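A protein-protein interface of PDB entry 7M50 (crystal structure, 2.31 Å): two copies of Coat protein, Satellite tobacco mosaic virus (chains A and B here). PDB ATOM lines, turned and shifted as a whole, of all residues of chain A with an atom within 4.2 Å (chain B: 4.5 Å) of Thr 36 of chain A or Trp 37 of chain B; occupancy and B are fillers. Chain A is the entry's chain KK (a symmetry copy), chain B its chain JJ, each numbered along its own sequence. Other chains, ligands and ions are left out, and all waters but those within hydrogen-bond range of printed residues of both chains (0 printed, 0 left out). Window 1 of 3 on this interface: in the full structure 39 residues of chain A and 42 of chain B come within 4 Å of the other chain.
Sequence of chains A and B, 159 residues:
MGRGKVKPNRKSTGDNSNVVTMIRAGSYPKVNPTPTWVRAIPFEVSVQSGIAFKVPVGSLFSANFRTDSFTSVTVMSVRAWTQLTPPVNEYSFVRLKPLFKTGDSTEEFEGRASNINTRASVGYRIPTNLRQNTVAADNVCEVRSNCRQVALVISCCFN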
ATOM      1  N   PRO A  35      17.357  14.601 -10.828  1.00  0.00           N
ATOM      2  CA  PRO A  35      16.722  14.491 -12.141  1.00  0.00           C
ATOM      3  C   PRO A  35      15.613  13.444 -12.126  1.00  0.00           C
ATOM      4  O   PRO A  35      15.279  12.864 -11.095  1.00  0.00           O
ATOM      5  CB  PRO A  35      17.881  14.071 -13.043  1.00  0.00           C
ATOM      6  CG  PRO A  35      18.743  13.246 -12.149  1.00  0.00           C
ATOM      7  CD  PRO A  35      18.631  13.862 -10.771  1.00  0.00           C
ATOM      8  N   THR A  36      15.040  13.214 -13.303  1.00  0.00           N
ATOM      9  CA  THR A  36      14.011  12.201 -13.469  1.00  0.00           C
ATOM     10  C   THR A  36      14.655  10.836 -13.697  1.00  0.00           C
ATOM     11  O   THR A  36      15.880  10.688 -13.696  1.00  0.00           O
ATOM     12  CB  THR A  36      13.083  12.568 -14.625  1.00  0.00           C
ATOM     13  OG1 THR A  36      13.850  12.701 -15.827  1.00  0.00           O
ATOM     14  CG2 THR A  36      12.372  13.877 -14.337  1.00  0.00           C
ATOM     15  N   TRP A  37      13.817   9.820 -13.904  1.00  0.00           N
ATOM     16  CA  TRP A  37      14.313   8.460 -14.100  1.00  0.00           C
ATOM     17  C   TRP A  37      13.200   7.606 -14.687  1.00  0.00           C
ATOM     18  O   TRP A  37      12.111   7.528 -14.109  1.00  0.00           O
ATOM     19  CB  TRP A  37      14.807   7.868 -12.777  1.00  0.00           C
ATOM     20  CG  TRP A  37      15.907   6.862 -12.932  1.00  0.00           C
ATOM     21  CD1 TRP A  37      16.467   6.430 -14.099  1.00  0.00           C
ATOM     22  CD2 TRP A  37      16.588   6.169 -11.879  1.00  0.00           C
ATOM     23  NE1 TRP A  37      17.452   5.507 -13.838  1.00  0.00           N
ATOM     24  CE2 TRP A  37      17.546   5.330 -12.483  1.00  0.00           C
ATOM     25  CE3 TRP A  37      16.480   6.173 -10.485  1.00  0.00           C
ATOM     26  CZ2 TRP A  37      18.389   4.504 -11.742  1.00  0.00           C
ATOM     27  CZ3 TRP A  37      17.318   5.353  -9.750  1.00  0.00           C
ATOM     28  CH2 TRP A  37      18.261   4.531 -10.381  1.00  0.00           C
ATOM     29  N   PHE A 158       9.799   8.270 -13.045  1.00  0.00           N
ATOM     30  CA  PHE A 158       9.844   8.968 -11.767  1.00  0.00           C
ATOM     31  C   PHE A 158      10.278  10.414 -11.958  1.00  0.00           C
ATOM     32  O   PHE A 158      11.224  10.704 -12.697  1.00  0.00           O
ATOM     33  CB  PHE A 158      10.794   8.258 -10.805  1.00  0.00           C
ATOM     34  CG  PHE A 158      10.294   6.925 -10.331  1.00  0.00           C
ATOM     35  CD1 PHE A 158       9.481   6.834  -9.213  1.00  0.00           C
ATOM     36  CD2 PHE A 158      10.638   5.762 -11.000  1.00  0.00           C
ATOM     37  CE1 PHE A 158       9.018   5.607  -8.771  1.00  0.00           C
ATOM     38  CE2 PHE A 158      10.181   4.533 -10.564  1.00  0.00           C
ATOM     39  CZ  PHE A 158       9.369   4.456  -9.448  1.00  0.00           C
ATOM     40  N   ASN A 159       9.582  11.325 -11.285  1.00  0.00           N
ATOM     41  CA  ASN A 159       9.903  12.745 -11.348  1.00  0.00           C
ATOM     42  C   ASN A 159       9.506  13.442 -10.050  1.00  0.00           C
ATOM     43  O   ASN A 159      10.076  14.468  -9.683  1.00  0.00           O
ATOM     44  CB  ASN A 159       9.204  13.406 -12.538  1.00  0.00           C
ATOM     45  CG  ASN A 159       7.699  13.455 -12.375  1.00  0.00           C
ATOM     46  OD1 ASN A 159       7.141  14.477 -11.975  1.00  0.00           O
ATOM     47  ND2 ASN A 159       7.031  12.349 -12.683  1.00  0.00           N
ATOM     48  OXT ASN A 159       8.609  12.994  -9.336  1.00  0.00           O
ATOM     49  N   PRO B  35      18.947  -0.783 -10.407  1.00  0.00           N
ATOM     50  CA  PRO B  35      19.810  -0.671 -11.586  1.00  0.00           C
ATOM     51  C   PRO B  35      20.885   0.394 -11.401  1.00  0.00           C
ATOM     52  O   PRO B  35      20.909   1.141 -10.422  1.00  0.00           O
ATOM     53  CB  PRO B  35      18.829  -0.279 -12.694  1.00  0.00           C
ATOM     54  CG  PRO B  35      17.790   0.519 -11.979  1.00  0.00           C
ATOM     55  CD  PRO B  35      17.658  -0.094 -10.601  1.00  0.00           C
ATOM     56  N   THR B  36      21.787   0.445 -12.378  1.00  0.00           N
ATOM     57  CA  THR B  36      22.845   1.442 -12.397  1.00  0.00           C
ATOM     58  C   THR B  36      22.278   2.799 -12.811  1.00  0.00           C
ATOM     59  O   THR B  36      21.096   2.937 -13.138  1.00  0.00           O
ATOM     60  CB  THR B  36      23.969   1.012 -13.336  1.00  0.00           C
ATOM     61  OG1 THR B  36      23.430   0.740 -14.636  1.00  0.00           O
ATOM     62  CG2 THR B  36      24.659  -0.235 -12.808  1.00  0.00           C
ATOM     63  N   TRP B  37      23.135   3.819 -12.802  1.00  0.00           N
ATOM     64  CA  TRP B  37      22.696   5.171 -13.138  1.00  0.00           C
ATOM     65  C   TRP B  37      23.908   6.001 -13.526  1.00  0.00           C
ATOM     66  O   TRP B  37      24.862   6.102 -12.748  1.00  0.00           O
ATOM     67  CB  TRP B  37      21.960   5.807 -11.958  1.00  0.00           C
ATOM     68  CG  TRP B  37      20.946   6.832 -12.361  1.00  0.00           C
ATOM     69  CD1 TRP B  37      20.655   7.244 -13.627  1.00  0.00           C
ATOM     70  CD2 TRP B  37      20.082   7.572 -11.489  1.00  0.00           C
ATOM     71  NE1 TRP B  37      19.665   8.196 -13.600  1.00  0.00           N
ATOM     72  CE2 TRP B  37      19.297   8.415 -12.299  1.00  0.00           C
ATOM     73  CE3 TRP B  37      19.900   7.604 -10.103  1.00  0.00           C
ATOM     74  CZ2 TRP B  37      18.342   9.281 -11.769  1.00  0.00           C
ATOM     75  CZ3 TRP B  37      18.952   8.464  -9.579  1.00  0.00           C
ATOM     76  CH2 TRP B  37      18.186   9.290 -10.410  1.00  0.00           C
ATOM     77  N   VAL B  38      23.873   6.589 -14.718  1.00  0.00           N
ATOM     78  CA  VAL B  38      24.901   7.526 -15.160  1.00  0.00           C
ATOM     79  C   VAL B  38      24.455   8.932 -14.782  1.00  0.00           C
ATOM     80  O   VAL B  38      23.320   9.332 -15.071  1.00  0.00           O
ATOM     81  CB  VAL B  38      25.144   7.408 -16.673  1.00  0.00           C
ATOM     82  CG1 VAL B  38      26.308   8.293 -17.092  1.00  0.00           C
ATOM     83  CG2 VAL B  38      25.404   5.962 -17.058  1.00  0.00           C
ATOM     84  N   ARG B  39      25.343   9.683 -14.134  1.00  0.00           N
ATOM     85  CA  ARG B  39      24.970  10.952 -13.528  1.00  0.00           C
ATOM     86  C   ARG B  39      26.093  11.968 -13.682  1.00  0.00           C
ATOM     87  O   ARG B  39      27.247  11.622 -13.949  1.00  0.00           O
ATOM     88  CB  ARG B  39      24.640  10.785 -12.038  1.00  0.00           C
ATOM     89  CG  ARG B  39      23.447   9.893 -11.745  1.00  0.00           C
ATOM     90  CD  ARG B  39      22.147  10.603 -12.069  1.00  0.00           C
ATOM     91  NE  ARG B  39      22.055  11.877 -11.367  1.00  0.00           N
ATOM     92  CZ  ARG B  39      21.652  12.012 -10.112  1.00  0.00           C
ATOM     93  NH1 ARG B  39      21.276  10.969  -9.390  1.00  0.00           N
ATOM     94  NH2 ARG B  39      21.629  13.225  -9.564  1.00  0.00           N
ATOM     95  N   ARG B  66      19.732  11.662  -4.936  1.00  0.00           N
ATOM     96  CA  ARG B  66      19.048  10.384  -5.146  1.00  0.00           C
ATOM     97  C   ARG B  66      20.036   9.225  -5.230  1.00  0.00           C
ATOM     98  O   ARG B  66      19.760   8.210  -5.873  1.00  0.00           O
ATOM     99  CB  ARG B  66      18.166  10.411  -6.400  1.00  0.00           C
ATOM    100  CG  ARG B  66      17.291  11.644  -6.559  1.00  0.00           C
ATOM    101  CD  ARG B  66      16.417  11.505  -7.797  1.00  0.00           C
ATOM    102  NE  ARG B  66      15.670  12.718  -8.110  1.00  0.00           N
ATOM    103  CZ  ARG B  66      14.488  13.025  -7.593  1.00  0.00           C
ATOM    104  NH1 ARG B  66      13.895  12.240  -6.708  1.00  0.00           N
ATOM    105  NH2 ARG B  66      13.884  14.148  -7.975  1.00  0.00           N
ATOM    106  N   PHE B  70      23.494   3.938  -3.108  1.00  0.00           N
ATOM    107  CA  PHE B  70      24.695   3.361  -3.689  1.00  0.00           C
ATOM    108  C   PHE B  70      25.828   3.327  -2.668  1.00  0.00           C
ATOM    109  O   PHE B  70      25.851   4.087  -1.697  1.00  0.00           O
ATOM    110  CB  PHE B  70      25.136   4.151  -4.922  1.00  0.00           C
ATOM    111  CG  PHE B  70      24.227   3.992  -6.106  1.00  0.00           C
ATOM    112  CD1 PHE B  70      24.432   2.972  -7.020  1.00  0.00           C
ATOM    113  CD2 PHE B  70      23.172   4.866  -6.309  1.00  0.00           C
ATOM    114  CE1 PHE B  70      23.601   2.825  -8.114  1.00  0.00           C
ATOM    115  CE2 PHE B  70      22.336   4.723  -7.401  1.00  0.00           C
ATOM    116  CZ  PHE B  70      22.551   3.702  -8.305  1.00  0.00           C
ATOM    117  N   CYS B 156      29.985  10.491 -13.648  1.00  0.00           N
ATOM    118  CA  CYS B 156      30.328   9.199 -13.075  1.00  0.00           C
ATOM    119  C   CYS B 156      29.212   8.206 -13.370  1.00  0.00           C
ATOM    120  O   CYS B 156      28.192   8.546 -13.980  1.00  0.00           O
ATOM    121  CB  CYS B 156      30.581   9.319 -11.567  1.00  0.00           C
ATOM    122  SG  CYS B 156      29.206  10.039 -10.638  1.00  0.00           S
ATOM    123  N   CYS B 157      29.412   6.966 -12.929  1.00  0.00           N
ATOM    124  CA  CYS B 157      28.456   5.879 -13.135  1.00  0.00           C
ATOM    125  C   CYS B 157      28.257   5.160 -11.804  1.00  0.00           C
ATOM    126  O   CYS B 157      29.104   4.363 -11.390  1.00  0.00           O
ATOM    127  CB  CYS B 157      28.943   4.915 -14.213  1.00  0.00           C
ATOM    128  SG  CYS B 157      29.167   5.653 -15.844  1.00  0.00           S
ATOM    129  N   PHE B 158      27.140   5.440 -11.139  1.00  0.00           N
ATOM    130  CA  PHE B 158      26.839   4.778  -9.877  1.00  0.00           C
ATOM    131  C   PHE B 158      26.450   3.325 -10.115  1.00  0.00           C
ATOM    132  O   PHE B 158      25.751   2.999 -11.078  1.00  0.00           O
ATOM    133  CB  PHE B 158      25.713   5.509  -9.148  1.00  0.00           C
ATOM    134  CG  PHE B 158      26.107   6.855  -8.612  1.00  0.00           C
ATOM    135  CD1 PHE B 158      26.714   6.970  -7.372  1.00  0.00           C
ATOM    136  CD2 PHE B 158      25.867   8.005  -9.344  1.00  0.00           C
ATOM    137  CE1 PHE B 158      27.078   8.207  -6.874  1.00  0.00           C
ATOM    138  CE2 PHE B 158      26.228   9.245  -8.852  1.00  0.00           C
ATOM    139  CZ  PHE B 158      26.835   9.346  -7.616  1.00  0.00           C
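Of the 5 printed residues of chain A, 3 touch a printed residue of chain B. Hydrophobic or aromatic side chains of chain A within 4 Å of the printed part of chain B: Pro 35 and Trp 37.
The guanidinium group (NE) of Arg 66 of chain B sits at hydrogen-bond distance from the backbone carbonyl oxygen (O) of Pro 35 of chain A, at 3.0 Å. The indole nitrogen of Trp 37 of chain A lies close to the indole nitrogen of Trp 37 of chain B, at 3.5 Å.
Of chain B, only Trp 37 (3.4 Å) comes within 4 Å of Thr 36 of chain A. Of the printed residues of chain B, Pro 35 of chain A touches Arg 39 and Arg 66. Of the printed residues of chain A, Thr 36 of chain B touches Trp 37 (3.4 Å). Printed residues of chain A within 4 Å of Arg 39 of chain B: Pro 35. Of the printed residues of chain A, Arg 66 of chain B touches Pro 35. Printed residues of chain B within 4 Å of Trp 37 of chain A: Thr 36 (3.4 Å) and Trp 37 (3.4 Å). Phe 158 of chain A touches none of the printed residues of chain B. Phe 158 of chain B touches none of the printed residues of chain A. The nearest printed residue of chain A that does not touch Trp 37 of chain B is Pro 35 of chain A (4.003 Å). The nearest printed residue of chain B that does not touch Trp 37 of chain A is Pro 35 of chain B (4.04 Å).
The backbone carbonyl oxygen (O) of Trp 37 of chain B lies within hydrogen-bond range of the backbone NH (N) of Phe 158 of chain B (2.9 Å). The backbone carbonyl oxygen (O) of Arg 39 of chain B sits at hydrogen-bond distance from the backbone NH (N) of Cys 156 of chain B (3.0 Å). O of Trp 37 of chain A sits at hydrogen-bond distance from N of Phe 158 of chain A (2.7 Å).
Arg 39 of chain B touches Pro 35 of chain A. Thr 36 of chain A touches Trp 37 of chain B (O to CZ2, 3.4 Å). Thr 36 of chain B touches Trp 37 of chain A (O to CZ2, 3.4 Å).
Thr 36 of chain A touches Trp 37 of chain B, and with the chains exchanged Trp 37 of chain A touches Thr 36 of chain B. Trp 37 of chain B touches its own counterpart, Trp 37 of chain A. Of the 5 pairs that touch across the chains among the printed residues, 3 have their exchanged pair printed and touching as well.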
